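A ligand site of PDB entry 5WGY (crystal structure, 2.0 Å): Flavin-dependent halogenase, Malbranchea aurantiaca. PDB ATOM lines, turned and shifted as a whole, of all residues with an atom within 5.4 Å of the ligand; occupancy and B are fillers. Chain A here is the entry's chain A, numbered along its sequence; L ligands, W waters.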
ATOM      1  N   PRO A  85     -25.006   0.896 -18.226  1.00  0.00           N
ATOM      2  CA  PRO A  85     -23.859   0.044 -17.877  1.00  0.00           C
ATOM      3  C   PRO A  85     -23.511  -1.018 -18.916  1.00  0.00           C
ATOM      4  O   PRO A  85     -22.331  -1.374 -19.059  1.00  0.00           O
ATOM      5  CB  PRO A  85     -24.300  -0.585 -16.538  1.00  0.00           C
ATOM      6  CG  PRO A  85     -25.188   0.506 -15.896  1.00  0.00           C
ATOM      7  CD  PRO A  85     -25.906   1.146 -17.079  1.00  0.00           C
ATOM      8  N   LEU A 111     -29.900   7.672 -12.413  1.00  0.00           N
ATOM      9  CA  LEU A 111     -31.116   8.128 -13.068  1.00  0.00           C
ATOM     10  C   LEU A 111     -31.981   8.792 -12.009  1.00  0.00           C
ATOM     11  O   LEU A 111     -32.112   8.269 -10.886  1.00  0.00           O
ATOM     12  CB  LEU A 111     -31.877   6.958 -13.709  1.00  0.00           C
ATOM     13  CG  LEU A 111     -31.187   6.079 -14.735  1.00  0.00           C
ATOM     14  CD1 LEU A 111     -32.184   5.097 -15.269  1.00  0.00           C
ATOM     15  CD2 LEU A 111     -30.743   6.925 -15.858  1.00  0.00           C
ATOM     16  N   SER A 129     -31.885   7.053  -8.217  1.00  0.00           N
ATOM     17  CA  SER A 129     -30.909   5.994  -8.084  1.00  0.00           C
ATOM     18  C   SER A 129     -29.540   6.557  -8.416  1.00  0.00           C
ATOM     19  O   SER A 129     -29.414   7.472  -9.232  1.00  0.00           O
ATOM     20  CB  SER A 129     -31.244   4.829  -9.003  1.00  0.00           C
ATOM     21  OG  SER A 129     -31.005   5.186 -10.340  1.00  0.00           O
ATOM     22  N   VAL A 130     -28.504   6.029  -7.757  1.00  0.00           N
ATOM     23  CA  VAL A 130     -27.119   6.328  -8.097  1.00  0.00           C
ATOM     24  C   VAL A 130     -26.631   5.262  -9.070  1.00  0.00           C
ATOM     25  O   VAL A 130     -27.301   4.242  -9.270  1.00  0.00           O
ATOM     26  CB  VAL A 130     -26.212   6.387  -6.851  1.00  0.00           C
ATOM     27  CG1 VAL A 130     -26.610   7.575  -5.963  1.00  0.00           C
ATOM     28  CG2 VAL A 130     -26.278   5.078  -6.070  1.00  0.00           C
ATOM     29  N   GLY A 131     -25.482   5.508  -9.702  1.00  0.00           N
ATOM     30  CA  GLY A 131     -24.792   4.511 -10.508  1.00  0.00           C
ATOM     31  C   GLY A 131     -23.887   3.606  -9.684  1.00  0.00           C
ATOM     32  O   GLY A 131     -24.393   2.777  -8.921  1.00  0.00           O
ATOM     33  N   ALA A 132     -22.575   3.750  -9.808  1.00  0.00           N
ATOM     34  CA  ALA A 132     -21.602   2.846  -9.206  1.00  0.00           C
ATOM     35  C   ALA A 132     -20.350   3.632  -8.856  1.00  0.00           C
ATOM     36  O   ALA A 132     -20.115   4.720  -9.416  1.00  0.00           O
ATOM     37  CB  ALA A 132     -21.248   1.694 -10.162  1.00  0.00           C
ATOM     38  N   PRO A 133     -19.518   3.119  -7.929  1.00  0.00           N
ATOM     39  CA  PRO A 133     -18.215   3.764  -7.674  1.00  0.00           C
ATOM     40  C   PRO A 133     -17.346   3.771  -8.931  1.00  0.00           C
ATOM     41  O   PRO A 133     -17.501   2.960  -9.843  1.00  0.00           O
ATOM     42  CB  PRO A 133     -17.590   2.895  -6.562  1.00  0.00           C
ATOM     43  CG  PRO A 133     -18.742   2.189  -5.911  1.00  0.00           C
ATOM     44  CD  PRO A 133     -19.784   1.996  -7.000  1.00  0.00           C
ATOM     45  N   VAL A 136     -15.821   0.612  -9.942  1.00  0.00           N
ATOM     46  CA  VAL A 136     -16.741  -0.438 -10.356  1.00  0.00           C
ATOM     47  C   VAL A 136     -17.070  -0.283 -11.844  1.00  0.00           C
ATOM     48  O   VAL A 136     -16.680  -1.124 -12.648  1.00  0.00           O
ATOM     49  CB  VAL A 136     -18.005  -0.430  -9.480  1.00  0.00           C
ATOM     50  CG1 VAL A 136     -19.037  -1.418 -10.043  1.00  0.00           C
ATOM     51  CG2 VAL A 136     -17.633  -0.792  -8.030  1.00  0.00           C
ATOM     52  N   LEU A 137     -17.795   0.785 -12.205  1.00  0.00           N
ATOM     53  CA  LEU A 137     -18.037   1.149 -13.602  1.00  0.00           C
ATOM     54  C   LEU A 137     -18.525   2.588 -13.686  1.00  0.00           C
ATOM     55  O   LEU A 137     -18.635   3.297 -12.672  1.00  0.00           O
ATOM     56  CB  LEU A 137     -19.019   0.176 -14.278  1.00  0.00           C
ATOM     57  CG  LEU A 137     -20.472   0.018 -13.815  1.00  0.00           C
ATOM     58  CD1 LEU A 137     -21.387   1.199 -14.257  1.00  0.00           C
ATOM     59  CD2 LEU A 137     -21.018  -1.316 -14.353  1.00  0.00           C
ATOM     60  N   TYR A 408     -35.574   5.595 -20.814  1.00  0.00           N
ATOM     61  CA  TYR A 408     -34.732   4.487 -20.367  1.00  0.00           C
ATOM     62  C   TYR A 408     -33.726   4.093 -21.441  1.00  0.00           C
ATOM     63  O   TYR A 408     -33.036   3.058 -21.289  1.00  0.00           O
ATOM     64  CB  TYR A 408     -35.517   3.243 -19.918  1.00  0.00           C
ATOM     65  CG  TYR A 408     -36.110   3.427 -18.552  1.00  0.00           C
ATOM     66  CD1 TYR A 408     -35.295   3.452 -17.429  1.00  0.00           C
ATOM     67  CD2 TYR A 408     -37.493   3.644 -18.382  1.00  0.00           C
ATOM     68  CE1 TYR A 408     -35.816   3.641 -16.159  1.00  0.00           C
ATOM     69  CE2 TYR A 408     -38.025   3.862 -17.108  1.00  0.00           C
ATOM     70  CZ  TYR A 408     -37.188   3.869 -16.009  1.00  0.00           C
ATOM     71  OH  TYR A 408     -37.707   4.096 -14.764  1.00  0.00           O
ATOM     72  N   GLN A 488     -39.141  -0.974 -13.078  1.00  0.00           N
ATOM     73  CA  GLN A 488     -38.152  -0.954 -14.150  1.00  0.00           C
ATOM     74  C   GLN A 488     -36.778  -1.241 -13.568  1.00  0.00           C
ATOM     75  O   GLN A 488     -35.953  -1.937 -14.166  1.00  0.00           O
ATOM     76  CB  GLN A 488     -38.122   0.411 -14.864  1.00  0.00           C
ATOM     77  CG  GLN A 488     -37.506   0.295 -16.252  1.00  0.00           C
ATOM     78  CD  GLN A 488     -38.489  -0.379 -17.211  1.00  0.00           C
ATOM     79  OE1 GLN A 488     -39.625   0.076 -17.358  1.00  0.00           O
ATOM     80  NE2 GLN A 488     -38.066  -1.486 -17.843  1.00  0.00           N
ATOM     81  N   PHE A 489     -36.519  -0.667 -12.406  1.00  0.00           N
ATOM     82  CA  PHE A 489     -35.268  -0.898 -11.705  1.00  0.00           C
ATOM     83  C   PHE A 489     -35.153  -2.345 -11.226  1.00  0.00           C
ATOM     84  O   PHE A 489     -34.120  -2.999 -11.425  1.00  0.00           O
ATOM     85  CB  PHE A 489     -35.174   0.089 -10.558  1.00  0.00           C
ATOM     86  CG  PHE A 489     -34.059  -0.165  -9.629  1.00  0.00           C
ATOM     87  CD1 PHE A 489     -32.745  -0.013 -10.044  1.00  0.00           C
ATOM     88  CD2 PHE A 489     -34.300  -0.537  -8.311  1.00  0.00           C
ATOM     89  CE1 PHE A 489     -31.688  -0.232  -9.165  1.00  0.00           C
ATOM     90  CE2 PHE A 489     -33.251  -0.760  -7.434  1.00  0.00           C
ATOM     91  CZ  PHE A 489     -31.944  -0.612  -7.860  1.00  0.00           C
ATOM     92  N   GLY A 492     -35.074  -4.736 -14.352  1.00  0.00           N
ATOM     93  CA  GLY A 492     -34.058  -4.456 -15.353  1.00  0.00           C
ATOM     94  C   GLY A 492     -32.638  -4.242 -14.867  1.00  0.00           C
ATOM     95  O   GLY A 492     -31.727  -4.047 -15.677  1.00  0.00           O
ATOM     96  N   ILE A 493     -32.406  -4.249 -13.554  1.00  0.00           N
ATOM     97  CA  ILE A 493     -31.020  -4.136 -13.085  1.00  0.00           C
ATOM     98  C   ILE A 493     -30.232  -5.329 -13.638  1.00  0.00           C
ATOM     99  O   ILE A 493     -30.767  -6.436 -13.804  1.00  0.00           O
ATOM    100  CB  ILE A 493     -30.961  -4.009 -11.551  1.00  0.00           C
ATOM    101  CG1 ILE A 493     -29.544  -3.684 -11.098  1.00  0.00           C
ATOM    102  CG2 ILE A 493     -31.443  -5.271 -10.847  1.00  0.00           C
ATOM    103  CD1 ILE A 493     -29.543  -2.770  -9.893  1.00  0.00           C
ATOM    104  N   GLU A 494     -28.975  -5.080 -14.005  1.00  0.00           N
ATOM    105  CA  GLU A 494     -28.211  -5.987 -14.864  1.00  0.00           C
ATOM    106  C   GLU A 494     -27.446  -6.959 -13.975  1.00  0.00           C
ATOM    107  O   GLU A 494     -26.234  -6.849 -13.767  1.00  0.00           O
ATOM    108  CB  GLU A 494     -27.273  -5.202 -15.785  1.00  0.00           C
ATOM    109  CG  GLU A 494     -27.954  -4.129 -16.633  1.00  0.00           C
ATOM    110  CD  GLU A 494     -27.917  -2.728 -16.022  1.00  0.00           C
ATOM    111  OE1 GLU A 494     -27.801  -2.627 -14.771  1.00  0.00           O
ATOM    112  OE2 GLU A 494     -27.985  -1.731 -16.792  1.00  0.00           O
ATOM    113  N   LEU A 497     -23.663  -8.727 -14.608  1.00  0.00           N
ATOM    114  CA  LEU A 497     -22.987  -8.022 -15.698  1.00  0.00           C
ATOM    115  C   LEU A 497     -21.465  -8.134 -15.576  1.00  0.00           C
ATOM    116  O   LEU A 497     -20.757  -8.170 -16.608  1.00  0.00           O
ATOM    117  CB  LEU A 497     -23.430  -6.549 -15.692  1.00  0.00           C
ATOM    118  CG  LEU A 497     -22.852  -5.495 -16.639  1.00  0.00           C
ATOM    119  CD1 LEU A 497     -23.246  -5.863 -18.054  1.00  0.00           C
ATOM    120  CD2 LEU A 497     -23.380  -4.055 -16.267  1.00  0.00           C
ATOM    121  N   TRP A 514     -34.112  -4.671 -20.743  1.00  0.00           N
ATOM    122  CA  TRP A 514     -34.499  -3.762 -19.655  1.00  0.00           C
ATOM    123  C   TRP A 514     -35.475  -4.405 -18.656  1.00  0.00           C
ATOM    124  O   TRP A 514     -36.235  -3.702 -17.970  1.00  0.00           O
ATOM    125  CB  TRP A 514     -35.109  -2.458 -20.221  1.00  0.00           C
ATOM    126  CG  TRP A 514     -34.246  -1.256 -19.973  1.00  0.00           C
ATOM    127  CD1 TRP A 514     -33.666  -0.436 -20.914  1.00  0.00           C
ATOM    128  CD2 TRP A 514     -33.861  -0.702 -18.694  1.00  0.00           C
ATOM    129  NE1 TRP A 514     -32.929   0.558 -20.301  1.00  0.00           N
ATOM    130  CE2 TRP A 514     -33.029   0.425 -18.943  1.00  0.00           C
ATOM    131  CE3 TRP A 514     -34.115  -1.075 -17.359  1.00  0.00           C
ATOM    132  CZ2 TRP A 514     -32.468   1.194 -17.914  1.00  0.00           C
ATOM    133  CZ3 TRP A 514     -33.572  -0.290 -16.325  1.00  0.00           C
ATOM    134  CH2 TRP A 514     -32.740   0.829 -16.614  1.00  0.00           C
ATOM    135  N   LEU A 568     -28.205  -7.561  -3.213  1.00  0.00           N
ATOM    136  CA  LEU A 568     -28.017  -6.171  -3.631  1.00  0.00           C
ATOM    137  C   LEU A 568     -28.385  -5.232  -2.479  1.00  0.00           C
ATOM    138  O   LEU A 568     -29.391  -5.452  -1.794  1.00  0.00           O
ATOM    139  CB  LEU A 568     -28.861  -5.884  -4.869  1.00  0.00           C
ATOM    140  CG  LEU A 568     -28.366  -4.675  -5.646  1.00  0.00           C
ATOM    141  CD1 LEU A 568     -27.473  -5.133  -6.741  1.00  0.00           C
ATOM    142  CD2 LEU A 568     -29.534  -3.914  -6.198  1.00  0.00           C
ATOM    143  N   ILE A 573     -28.708   2.145  -3.148  1.00  0.00           N
ATOM    144  CA  ILE A 573     -28.856   2.575  -4.539  1.00  0.00           C
ATOM    145  C   ILE A 573     -30.073   3.482  -4.757  1.00  0.00           C
ATOM    146  O   ILE A 573     -29.979   4.465  -5.495  1.00  0.00           O
ATOM    147  CB  ILE A 573     -28.925   1.324  -5.424  1.00  0.00           C
ATOM    148  CG1 ILE A 573     -27.688   0.486  -5.167  1.00  0.00           C
ATOM    149  CG2 ILE A 573     -29.143   1.732  -6.912  1.00  0.00           C
ATOM    150  CD1 ILE A 573     -27.757  -0.868  -5.812  1.00  0.00           C
ATOM    151  N   TYR A 593     -21.101   8.581  -4.885  1.00  0.00           N
ATOM    152  CA  TYR A 593     -20.042   8.153  -5.786  1.00  0.00           C
ATOM    153  C   TYR A 593     -19.383   9.278  -6.565  1.00  0.00           C
ATOM    154  O   TYR A 593     -18.386   9.003  -7.240  1.00  0.00           O
ATOM    155  CB  TYR A 593     -20.578   7.145  -6.814  1.00  0.00           C
ATOM    156  CG  TYR A 593     -21.189   5.897  -6.196  1.00  0.00           C
ATOM    157  CD1 TYR A 593     -20.703   5.373  -5.001  1.00  0.00           C
ATOM    158  CD2 TYR A 593     -22.271   5.268  -6.811  1.00  0.00           C
ATOM    159  CE1 TYR A 593     -21.284   4.213  -4.427  1.00  0.00           C
ATOM    160  CE2 TYR A 593     -22.854   4.124  -6.260  1.00  0.00           C
ATOM    161  CZ  TYR A 593     -22.356   3.602  -5.072  1.00  0.00           C
ATOM    162  OH  TYR A 593     -22.941   2.483  -4.556  1.00  0.00           O
ATOM    163  N   LEU A 641     -15.860  -5.766  -3.482  1.00  0.00           N
ATOM    164  CA  LEU A 641     -16.649  -5.124  -4.538  1.00  0.00           C
ATOM    165  C   LEU A 641     -15.779  -4.751  -5.740  1.00  0.00           C
ATOM    166  O   LEU A 641     -16.068  -5.116  -6.881  1.00  0.00           O
ATOM    167  CB  LEU A 641     -17.376  -3.897  -3.974  1.00  0.00           C
ATOM    168  CG  LEU A 641     -18.131  -2.968  -4.939  1.00  0.00           C
ATOM    169  CD1 LEU A 641     -19.184  -3.719  -5.730  1.00  0.00           C
ATOM    170  CD2 LEU A 641     -18.781  -1.825  -4.170  1.00  0.00           C
ATOM    171  N   TRP A 645     -15.027  -6.371 -10.276  1.00  0.00           N
ATOM    172  CA  TRP A 645     -15.204  -5.586 -11.496  1.00  0.00           C
ATOM    173  C   TRP A 645     -13.902  -5.200 -12.178  1.00  0.00           C
ATOM    174  O   TRP A 645     -13.898  -4.368 -13.098  1.00  0.00           O
ATOM    175  CB  TRP A 645     -15.988  -4.323 -11.147  1.00  0.00           C
ATOM    176  CG  TRP A 645     -17.383  -4.640 -10.776  1.00  0.00           C
ATOM    177  CD1 TRP A 645     -17.869  -4.959  -9.525  1.00  0.00           C
ATOM    178  CD2 TRP A 645     -18.503  -4.680 -11.663  1.00  0.00           C
ATOM    179  NE1 TRP A 645     -19.236  -5.170  -9.594  1.00  0.00           N
ATOM    180  CE2 TRP A 645     -19.643  -4.995 -10.897  1.00  0.00           C
ATOM    181  CE3 TRP A 645     -18.644  -4.473 -13.048  1.00  0.00           C
ATOM    182  CZ2 TRP A 645     -20.926  -5.124 -11.462  1.00  0.00           C
ATOM    183  CZ3 TRP A 645     -19.921  -4.590 -13.613  1.00  0.00           C
ATOM    184  CH2 TRP A 645     -21.041  -4.914 -12.820  1.00  0.00           C
HETATM  185  N1  LIG L   1     -23.967   0.007  -8.663  1.00  0.00           N
HETATM  186  C1  LIG L   1     -22.923  -0.781  -8.357  1.00  0.00           C
HETATM  187  O1  LIG L   1     -21.911  -0.360  -7.809  1.00  0.00           O
HETATM  188  C2  LIG L   1     -23.108  -2.238  -8.781  1.00  0.00           C
HETATM  189  C3  LIG L   1     -30.679   1.104 -12.440  1.00  0.00           C
HETATM  190  C4  LIG L   1     -29.889   0.113 -13.004  1.00  0.00           C
HETATM  191  C5  LIG L   1     -28.665  -0.168 -12.398  1.00  0.00           C
HETATM  192  C6  LIG L   1     -26.639  -0.972 -11.803  1.00  0.00           C
HETATM  193  C7  LIG L   1     -25.377  -1.805 -11.779  1.00  0.00           C
HETATM  194  C8  LIG L   1     -25.789  -3.276 -11.553  1.00  0.00           C
HETATM  195  C9  LIG L   1     -24.664  -1.709 -13.136  1.00  0.00           C
HETATM  196  C10 LIG L   1     -25.517  -1.791  -8.395  1.00  0.00           C
HETATM  197  C11 LIG L   1     -24.024  -3.023  -6.808  1.00  0.00           C
HETATM  198  C12 LIG L   1     -22.692  -3.740  -6.915  1.00  0.00           C
HETATM  199  C13 LIG L   1     -23.275  -2.251 -10.314  1.00  0.00           C
HETATM  200  C14 LIG L   1     -22.048  -3.190  -8.193  1.00  0.00           C
HETATM  201  C15 LIG L   1     -24.417  -1.270 -10.666  1.00  0.00           C
HETATM  202  C16 LIG L   1     -25.069  -0.676  -9.350  1.00  0.00           C
HETATM  203  C17 LIG L   1     -26.097   0.394  -9.725  1.00  0.00           C
HETATM  204  C18 LIG L   1     -26.958  -0.008 -10.880  1.00  0.00           C
HETATM  205  C19 LIG L   1     -28.241   0.525 -11.249  1.00  0.00           C
HETATM  206  C20 LIG L   1     -29.066   1.517 -10.725  1.00  0.00           C
HETATM  207  C21 LIG L   1     -30.278   1.814 -11.320  1.00  0.00           C
HETATM  208  N2  LIG L   1     -27.662  -1.073 -12.731  1.00  0.00           N
HETATM  209  N3  LIG L   1     -24.398  -2.715  -8.200  1.00  0.00           N
HETATM  210 CL1  LIG L   1     -32.278   1.388 -13.088  1.00  0.00          CL
HETATM  211  O   HOH W   1     -29.305   0.482 -15.978  1.00  0.00           O
HETATM  212  O   HOH W   2     -24.754  -4.075  -3.608  1.00  0.00           O
HETATM  213  O   HOH W   3     -24.905  -5.479  -8.974  1.00  0.00           O
HETATM  214  O   HOH W   4     -21.947  -0.119  -4.870  1.00  0.00           O
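Water W4 bridges OH of Tyr 593 (2.8 Å) and O1 of the ligand (2.9 Å).
N of Ser 129 lies within hydrogen-bond range of O of Leu 111 (2.9 Å).
O of Tyr 408 is in hydrogen-bond range of NE1 of Trp 514, 2.7 Å away.
The backbone NH of Val 130 lies within hydrogen-bond range of the backbone carbonyl oxygen of Ile 573.
O of Trp 514 sits at hydrogen-bond distance from NE2 of Gln 488 (2.9 Å).
Pro 85 touches the ligand (CG to C9, 3.6 Å).
OG of Ser 129 touches C21 of the ligand, 3.6 Å away.
O of Val 130 touches C20 of the ligand, 3.6 Å away.
Ala 132 touches the ligand.
Pro 133 touches the ligand (CD to O1, 3.3 Å).
Val 136 touches the ligand.
Leu 137 touches the ligand.
Phe 489 touches the ligand (CE1 to C21, 3.3 Å).
CG1 of Ile 493 touches N2 of the ligand, at 3.6 Å.
Trp 514 touches the ligand (CH2 to CL1, 3.6 Å).
Ile 573 touches the ligand (CD1 to C10, 3.5 Å).
CD1 of Leu 641 touches C12 of the ligand (3.7 Å).
Trp 645 touches the ligand.
Hydrophobic or aromatic side chains within 4 Å of the ligand: Pro 85, Ala 132, Pro 133, Val 136, Leu 137, Phe 489, Ile 493, Trp 514, Ile 573, Leu 641 and Trp 645.
15 residues have an atom within 4 Å of the ligand: Pro 85, Ser 129, Val 130, Gly 131, Ala 132, Pro 133, Val 136, Leu 137, Phe 489, Ile 493, Glu 494, Trp 514, Ile 573, Leu 641 and Trp 645.
The backbone carbonyl oxygen (O) of Gly 131 sits at hydrogen-bond distance from a nitrogen (N1) of the ligand (2.8 Å).
The side-chain carboxylate of Glu 494 sits at hydrogen-bond distance from a nitrogen (N2) of the ligand.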
